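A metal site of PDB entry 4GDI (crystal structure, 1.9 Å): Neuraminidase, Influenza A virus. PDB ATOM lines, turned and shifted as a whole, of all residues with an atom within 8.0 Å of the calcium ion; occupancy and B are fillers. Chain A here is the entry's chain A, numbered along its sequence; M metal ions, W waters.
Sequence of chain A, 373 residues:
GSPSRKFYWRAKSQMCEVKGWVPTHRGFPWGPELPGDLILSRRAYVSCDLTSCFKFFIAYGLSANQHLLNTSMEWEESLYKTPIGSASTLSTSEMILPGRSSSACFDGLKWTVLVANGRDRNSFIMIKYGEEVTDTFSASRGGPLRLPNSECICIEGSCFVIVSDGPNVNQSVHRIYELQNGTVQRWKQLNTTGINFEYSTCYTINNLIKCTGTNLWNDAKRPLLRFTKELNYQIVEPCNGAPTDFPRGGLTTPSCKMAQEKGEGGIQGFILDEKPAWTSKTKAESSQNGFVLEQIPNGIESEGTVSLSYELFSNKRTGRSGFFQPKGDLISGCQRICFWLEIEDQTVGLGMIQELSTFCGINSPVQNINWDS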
ATOM      1  N   ASN A 196       3.462  31.268  -5.665  1.00  0.00           N
ATOM      2  CA  ASN A 196       4.429  32.282  -6.079  1.00  0.00           C
ATOM      3  C   ASN A 196       3.674  33.246  -6.992  1.00  0.00           C
ATOM      4  O   ASN A 196       2.837  32.808  -7.771  1.00  0.00           O
ATOM      5  CB  ASN A 196       5.604  31.609  -6.810  1.00  0.00           C
ATOM      6  CG  ASN A 196       6.557  32.591  -7.446  1.00  0.00           C
ATOM      7  OD1 ASN A 196       6.748  32.593  -8.656  1.00  0.00           O
ATOM      8  ND2 ASN A 196       7.187  33.421  -6.629  1.00  0.00           N
ATOM      9  N   GLY A 213      -0.998  37.232 -11.967  1.00  0.00           N
ATOM     10  CA  GLY A 213       0.359  36.838 -11.636  1.00  0.00           C
ATOM     11  C   GLY A 213       0.898  35.711 -12.494  1.00  0.00           C
ATOM     12  O   GLY A 213       0.194  35.151 -13.343  1.00  0.00           O
ATOM     13  N   THR A 214       2.176  35.411 -12.297  1.00  0.00           N
ATOM     14  CA  THR A 214       2.812  34.256 -12.911  1.00  0.00           C
ATOM     15  C   THR A 214       3.441  33.457 -11.775  1.00  0.00           C
ATOM     16  O   THR A 214       4.231  33.982 -10.997  1.00  0.00           O
ATOM     17  CB  THR A 214       3.877  34.675 -13.910  1.00  0.00           C
ATOM     18  OG1 THR A 214       3.256  35.323 -15.017  1.00  0.00           O
ATOM     19  CG2 THR A 214       4.676  33.431 -14.431  1.00  0.00           C
ATOM     20  N   ASN A 215       3.029  32.194 -11.634  1.00  0.00           N
ATOM     21  CA  ASN A 215       3.581  31.326 -10.601  1.00  0.00           C
ATOM     22  C   ASN A 215       4.724  30.511 -11.190  1.00  0.00           C
ATOM     23  O   ASN A 215       4.505  29.612 -11.998  1.00  0.00           O
ATOM     24  CB  ASN A 215       2.496  30.397 -10.046  1.00  0.00           C
ATOM     25  CG  ASN A 215       2.964  29.589  -8.839  1.00  0.00           C
ATOM     26  OD1 ASN A 215       4.140  29.235  -8.735  1.00  0.00           O
ATOM     27  ND2 ASN A 215       2.050  29.283  -7.936  1.00  0.00           N
ATOM     28  N   LEU A 216       5.955  30.834 -10.780  1.00  0.00           N
ATOM     29  CA  LEU A 216       7.156  30.213 -11.350  1.00  0.00           C
ATOM     30  C   LEU A 216       7.556  28.940 -10.592  1.00  0.00           C
ATOM     31  O   LEU A 216       8.530  28.267 -10.940  1.00  0.00           O
ATOM     32  CB  LEU A 216       8.322  31.208 -11.286  1.00  0.00           C
ATOM     33  CG  LEU A 216       8.197  32.468 -12.136  1.00  0.00           C
ATOM     34  CD1 LEU A 216       9.465  33.325 -12.006  1.00  0.00           C
ATOM     35  CD2 LEU A 216       7.938  32.120 -13.598  1.00  0.00           C
ATOM     36  N   TRP A 217       6.796  28.631  -9.560  1.00  0.00           N
ATOM     37  CA  TRP A 217       7.137  27.567  -8.631  1.00  0.00           C
ATOM     38  C   TRP A 217       6.357  26.290  -8.915  1.00  0.00           C
ATOM     39  O   TRP A 217       6.926  25.284  -9.350  1.00  0.00           O
ATOM     40  CB  TRP A 217       6.838  28.041  -7.207  1.00  0.00           C
ATOM     41  CG  TRP A 217       6.979  27.004  -6.170  1.00  0.00           C
ATOM     42  CD1 TRP A 217       7.640  25.808  -6.281  1.00  0.00           C
ATOM     43  CD2 TRP A 217       6.446  27.052  -4.844  1.00  0.00           C
ATOM     44  NE1 TRP A 217       7.557  25.110  -5.099  1.00  0.00           N
ATOM     45  CE2 TRP A 217       6.818  25.845  -4.201  1.00  0.00           C
ATOM     46  CE3 TRP A 217       5.681  27.981  -4.128  1.00  0.00           C
ATOM     47  CZ2 TRP A 217       6.462  25.560  -2.895  1.00  0.00           C
ATOM     48  CZ3 TRP A 217       5.333  27.697  -2.834  1.00  0.00           C
ATOM     49  CH2 TRP A 217       5.717  26.492  -2.226  1.00  0.00           C
ATOM     50  N   ASN A 218       5.041  26.336  -8.680  1.00  0.00           N
ATOM     51  CA  ASN A 218       4.225  25.131  -8.679  1.00  0.00           C
ATOM     52  C   ASN A 218       2.838  25.292  -9.290  1.00  0.00           C
ATOM     53  O   ASN A 218       1.890  24.677  -8.821  1.00  0.00           O
ATOM     54  CB  ASN A 218       4.044  24.665  -7.235  1.00  0.00           C
ATOM     55  CG  ASN A 218       3.465  25.753  -6.358  1.00  0.00           C
ATOM     56  OD1 ASN A 218       3.100  26.827  -6.837  1.00  0.00           O
ATOM     57  ND2 ASN A 218       3.367  25.478  -5.056  1.00  0.00           N
ATOM     58  N   ASP A 219       2.704  26.115 -10.333  1.00  0.00           N
ATOM     59  CA  ASP A 219       1.393  26.275 -10.966  1.00  0.00           C
ATOM     60  C   ASP A 219       1.488  26.712 -12.398  1.00  0.00           C
ATOM     61  O   ASP A 219       2.274  27.598 -12.742  1.00  0.00           O
ATOM     62  CB  ASP A 219       0.508  27.270 -10.185  1.00  0.00           C
ATOM     63  CG  ASP A 219      -0.979  27.124 -10.481  1.00  0.00           C
ATOM     64  OD1 ASP A 219      -1.380  26.300 -11.343  1.00  0.00           O
ATOM     65  OD2 ASP A 219      -1.785  27.849  -9.852  1.00  0.00           O
ATOM     66  N   ALA A 220       0.660  26.089 -13.224  1.00  0.00           N
ATOM     67  CA  ALA A 220       0.552  26.448 -14.625  1.00  0.00           C
ATOM     68  C   ALA A 220      -0.742  27.217 -14.880  1.00  0.00           C
ATOM     69  O   ALA A 220      -0.983  27.699 -15.976  1.00  0.00           O
ATOM     70  CB  ALA A 220       0.623  25.172 -15.504  1.00  0.00           C
ATOM     71  N   LYS A 221      -1.594  27.303 -13.863  1.00  0.00           N
ATOM     72  CA  LYS A 221      -2.660  28.295 -13.908  1.00  0.00           C
ATOM     73  C   LYS A 221      -2.024  29.590 -13.447  1.00  0.00           C
ATOM     74  O   LYS A 221      -0.952  29.568 -12.826  1.00  0.00           O
ATOM     75  CB  LYS A 221      -3.827  27.916 -12.985  1.00  0.00           C
ATOM     76  CG  LYS A 221      -4.875  27.015 -13.641  1.00  0.00           C
ATOM     77  CD  LYS A 221      -5.861  26.502 -12.607  1.00  0.00           C
ATOM     78  CE  LYS A 221      -6.926  25.605 -13.249  1.00  0.00           C
ATOM     79  NZ  LYS A 221      -7.975  25.212 -12.280  1.00  0.00           N
ATOM     80  N   ARG A 222      -2.644  30.719 -13.752  1.00  0.00           N
ATOM     81  CA  ARG A 222      -2.140  32.003 -13.268  1.00  0.00           C
ATOM     82  C   ARG A 222      -2.994  32.422 -12.086  1.00  0.00           C
ATOM     83  O   ARG A 222      -4.203  32.504 -12.215  1.00  0.00           O
ATOM     84  CB  ARG A 222      -2.217  33.060 -14.361  1.00  0.00           C
ATOM     85  CG  ARG A 222      -1.409  32.716 -15.590  1.00  0.00           C
ATOM     86  CD  ARG A 222      -1.481  33.820 -16.612  1.00  0.00           C
ATOM     87  NE  ARG A 222      -0.663  33.566 -17.788  1.00  0.00           N
ATOM     88  CZ  ARG A 222       0.653  33.730 -17.822  1.00  0.00           C
ATOM     89  NH1 ARG A 222       1.308  34.116 -16.732  1.00  0.00           N
ATOM     90  NH2 ARG A 222       1.332  33.492 -18.945  1.00  0.00           N
ATOM     91  N   PRO A 223      -2.357  32.655 -10.934  1.00  0.00           N
ATOM     92  CA  PRO A 223      -3.093  33.193  -9.783  1.00  0.00           C
ATOM     93  C   PRO A 223      -3.555  34.617 -10.052  1.00  0.00           C
ATOM     94  O   PRO A 223      -2.922  35.371 -10.808  1.00  0.00           O
ATOM     95  CB  PRO A 223      -2.058  33.169  -8.660  1.00  0.00           C
ATOM     96  CG  PRO A 223      -0.746  33.283  -9.360  1.00  0.00           C
ATOM     97  CD  PRO A 223      -0.907  32.581 -10.688  1.00  0.00           C
ATOM     98  N   THR A 244      -2.991  28.629 -18.386  1.00  0.00           N
ATOM     99  CA  THR A 244      -2.562  29.594 -19.408  1.00  0.00           C
ATOM    100  C   THR A 244      -1.118  30.054 -19.295  1.00  0.00           C
ATOM    101  O   THR A 244      -0.652  30.833 -20.116  1.00  0.00           O
ATOM    102  CB  THR A 244      -3.484  30.849 -19.441  1.00  0.00           C
ATOM    103  OG1 THR A 244      -3.392  31.576 -18.208  1.00  0.00           O
ATOM    104  CG2 THR A 244      -4.915  30.471 -19.715  1.00  0.00           C
ATOM    105  N   ASP A 245      -0.403  29.569 -18.287  1.00  0.00           N
ATOM    106  CA  ASP A 245       1.016  29.845 -18.185  1.00  0.00           C
ATOM    107  C   ASP A 245       1.733  29.101 -19.325  1.00  0.00           C
ATOM    108  O   ASP A 245       1.165  28.244 -19.997  1.00  0.00           O
ATOM    109  CB  ASP A 245       1.535  29.371 -16.833  1.00  0.00           C
ATOM    110  CG  ASP A 245       2.786  30.099 -16.378  1.00  0.00           C
ATOM    111  OD1 ASP A 245       3.316  30.962 -17.122  1.00  0.00           O
ATOM    112  OD2 ASP A 245       3.245  29.790 -15.256  1.00  0.00           O
ATOM    113  N   PHE A 246       2.983  29.470 -19.572  1.00  0.00           N
ATOM    114  CA  PHE A 246       3.871  28.644 -20.380  1.00  0.00           C
ATOM    115  C   PHE A 246       5.197  28.528 -19.641  1.00  0.00           C
ATOM    116  O   PHE A 246       5.811  29.534 -19.314  1.00  0.00           O
ATOM    117  CB  PHE A 246       4.103  29.210 -21.773  1.00  0.00           C
ATOM    118  CG  PHE A 246       4.801  28.242 -22.681  1.00  0.00           C
ATOM    119  CD1 PHE A 246       6.182  28.077 -22.615  1.00  0.00           C
ATOM    120  CD2 PHE A 246       4.081  27.435 -23.547  1.00  0.00           C
ATOM    121  CE1 PHE A 246       6.836  27.151 -23.408  1.00  0.00           C
ATOM    122  CE2 PHE A 246       4.731  26.509 -24.354  1.00  0.00           C
ATOM    123  CZ  PHE A 246       6.106  26.372 -24.280  1.00  0.00           C
ATOM    124  N   PRO A 247       5.649  27.277 -19.407  1.00  0.00           N
ATOM    125  CA  PRO A 247       5.049  26.027 -19.908  1.00  0.00           C
ATOM    126  C   PRO A 247       3.795  25.630 -19.163  1.00  0.00           C
ATOM    127  O   PRO A 247       3.422  26.261 -18.160  1.00  0.00           O
ATOM    128  CB  PRO A 247       6.149  24.989 -19.661  1.00  0.00           C
ATOM    129  CG  PRO A 247       6.874  25.495 -18.468  1.00  0.00           C
ATOM    130  CD  PRO A 247       6.817  27.012 -18.537  1.00  0.00           C
ATOM    131  N   ARG A 248       3.140  24.571 -19.653  1.00  0.00           N
ATOM    132  CA  ARG A 248       1.959  24.038 -18.990  1.00  0.00           C
ATOM    133  C   ARG A 248       1.702  22.617 -19.473  1.00  0.00           C
ATOM    134  O   ARG A 248       2.262  22.202 -20.470  1.00  0.00           O
ATOM    135  CB  ARG A 248       0.718  24.889 -19.294  1.00  0.00           C
ATOM    136  CG  ARG A 248       0.390  25.038 -20.770  1.00  0.00           C
ATOM    137  CD  ARG A 248      -0.987  25.675 -20.940  1.00  0.00           C
ATOM    138  NE  ARG A 248      -1.387  25.839 -22.336  1.00  0.00           N
ATOM    139  CZ  ARG A 248      -0.918  26.775 -23.167  1.00  0.00           C
ATOM    140  NH1 ARG A 248       0.004  27.658 -22.765  1.00  0.00           N
ATOM    141  NH2 ARG A 248      -1.374  26.810 -24.412  1.00  0.00           N
ATOM    142  N   ALA A 259      -3.008  23.843 -11.288  1.00  0.00           N
ATOM    143  CA  ALA A 259      -2.535  22.922 -12.322  1.00  0.00           C
ATOM    144  C   ALA A 259      -1.037  22.708 -12.124  1.00  0.00           C
ATOM    145  O   ALA A 259      -0.207  23.442 -12.637  1.00  0.00           O
ATOM    146  CB  ALA A 259      -2.814  23.508 -13.690  1.00  0.00           C
ATOM    147  N   GLN A 260      -0.691  21.679 -11.367  1.00  0.00           N
ATOM    148  CA  GLN A 260       0.702  21.499 -10.978  1.00  0.00           C
ATOM    149  C   GLN A 260       1.557  20.854 -12.064  1.00  0.00           C
ATOM    150  O   GLN A 260       2.777  20.942 -12.010  1.00  0.00           O
ATOM    151  CB  GLN A 260       0.788  20.742  -9.669  1.00  0.00           C
ATOM    152  CG  GLN A 260      -0.262  21.210  -8.671  1.00  0.00           C
ATOM    153  CD  GLN A 260       0.258  21.324  -7.254  1.00  0.00           C
ATOM    154  OE1 GLN A 260       0.865  22.330  -6.879  1.00  0.00           O
ATOM    155  NE2 GLN A 260       0.006  20.294  -6.443  1.00  0.00           N
ATOM    156  N   GLU A 261       0.934  20.240 -13.071  1.00  0.00           N
ATOM    157  CA  GLU A 261       1.719  19.644 -14.162  1.00  0.00           C
ATOM    158  C   GLU A 261       2.520  20.728 -14.881  1.00  0.00           C
ATOM    159  O   GLU A 261       1.941  21.628 -15.508  1.00  0.00           O
ATOM    160  CB  GLU A 261       0.834  18.891 -15.172  1.00  0.00           C
ATOM    161  CG  GLU A 261       1.657  18.090 -16.199  1.00  0.00           C
ATOM    162  CD  GLU A 261       0.825  17.553 -17.371  1.00  0.00           C
ATOM    163  OE1 GLU A 261      -0.413  17.719 -17.378  1.00  0.00           O
ATOM    164  OE2 GLU A 261       1.434  16.975 -18.310  1.00  0.00           O
ATOM    165  N   LYS A 262       3.844  20.637 -14.789  1.00  0.00           N
ATOM    166  CA  LYS A 262       4.755  21.602 -15.415  1.00  0.00           C
ATOM    167  C   LYS A 262       4.510  23.010 -14.894  1.00  0.00           C
ATOM    168  O   LYS A 262       4.553  23.979 -15.649  1.00  0.00           O
ATOM    169  CB  LYS A 262       4.640  21.540 -16.934  1.00  0.00           C
ATOM    170  CG  LYS A 262       5.237  20.252 -17.510  1.00  0.00           C
ATOM    171  CD  LYS A 262       4.644  19.902 -18.855  1.00  0.00           C
ATOM    172  CE  LYS A 262       5.476  20.453 -20.005  1.00  0.00           C
ATOM    173  NZ  LYS A 262       4.786  20.248 -21.313  1.00  0.00           N
ATOM    174  N   GLY A 263       4.264  23.112 -13.599  1.00  0.00           N
ATOM    175  CA  GLY A 263       3.964  24.380 -12.973  1.00  0.00           C
ATOM    176  C   GLY A 263       5.206  25.211 -12.740  1.00  0.00           C
ATOM    177  O   GLY A 263       5.128  26.418 -12.540  1.00  0.00           O
ATOM    178  N   GLU A 264       6.368  24.557 -12.767  1.00  0.00           N
ATOM    179  CA  GLU A 264       7.620  25.261 -12.538  1.00  0.00           C
ATOM    180  C   GLU A 264       7.925  26.110 -13.748  1.00  0.00           C
ATOM    181  O   GLU A 264       7.615  25.716 -14.875  1.00  0.00           O
ATOM    182  CB  GLU A 264       8.763  24.274 -12.288  1.00  0.00           C
ATOM    183  CG  GLU A 264      10.009  24.938 -11.743  1.00  0.00           C
ATOM    184  CD  GLU A 264      11.159  23.946 -11.533  1.00  0.00           C
ATOM    185  OE1 GLU A 264      10.937  22.730 -11.645  1.00  0.00           O
ATOM    186  OE2 GLU A 264      12.290  24.414 -11.259  1.00  0.00           O
ATOM    187  N   GLY A 265       8.520  27.277 -13.530  1.00  0.00           N
ATOM    188  CA  GLY A 265       8.765  28.212 -14.607  1.00  0.00           C
ATOM    189  C   GLY A 265       7.488  28.930 -15.033  1.00  0.00           C
ATOM    190  O   GLY A 265       6.429  28.749 -14.430  1.00  0.00           O
ATOM    191  N   GLY A 266       7.593  29.742 -16.071  1.00  0.00           N
ATOM    192  CA  GLY A 266       6.466  30.491 -16.565  1.00  0.00           C
ATOM    193  C   GLY A 266       6.867  31.780 -17.244  1.00  0.00           C
ATOM    194  O   GLY A 266       8.053  32.090 -17.402  1.00  0.00           O
ATOM    195  N   ILE A 267       5.854  32.544 -17.648  1.00  0.00           N
ATOM    196  CA  ILE A 267       6.072  33.745 -18.424  1.00  0.00           C
ATOM    197  C   ILE A 267       4.943  34.736 -18.140  1.00  0.00           C
ATOM    198  O   ILE A 267       3.800  34.339 -17.956  1.00  0.00           O
ATOM    199  CB  ILE A 267       6.169  33.408 -19.920  1.00  0.00           C
ATOM    200  CG1 ILE A 267       6.725  34.606 -20.693  1.00  0.00           C
ATOM    201  CG2 ILE A 267       4.812  32.957 -20.441  1.00  0.00           C
ATOM    202  CD1 ILE A 267       7.125  34.313 -22.129  1.00  0.00           C
HETATM  203 CA    CA M   1       4.201  28.307 -13.831  1.00  0.00          CA
HETATM  204  O   HOH W   1       4.078  26.700 -15.650  1.00  0.00           O
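N of Asp 245 is in hydrogen-bond range of O of Ala 220. The backbone NH of Ile 267 sits at hydrogen-bond distance from the side-chain carboxylate of Asp 245 (3.0 Å). The backbone carbonyl oxygen of Asp 245 sits at hydrogen-bond distance from the guanidinium group of Arg 248, 3.1 Å away. OD1 of Asp 245 lies within salt-bridge range of NH2 of Arg 222, at 3.7 Å. The backbone NH (N) of Trp 217 is in hydrogen-bond range of the side-chain amide oxygen (OD1) of Asn 215 (2.8 Å). The side-chain amide nitrogen (ND2) of Asn 215 lies within hydrogen-bond range of the side-chain amide oxygen (OD1) of Asn 218. The side-chain amide nitrogen (ND2) of Asn 215 lies close to the backbone NH (N) of Asn 196, 3.3 Å away. The side-chain carboxylate of Asp 219 sits at hydrogen-bond distance from the backbone NH of Ala 259, 2.9 Å away.
Water W1 lies within hydrogen-bond range of O of Pro 247 (2.6 Å) and O of Lys 262 (2.8 Å).
The calcium ion is bound by OD2 of Asp 245, O of Asn 215, O of Asp 219, O of Gly 265, water W1 and O of Gly 263. The calcium ion has six donor atoms within binding distance.
Of the 26 residues printed, 5 come within 4 Å of the calcium ion. The nearest printed residue that does not touch the calcium ion is Gly 266 (4.2 Å).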
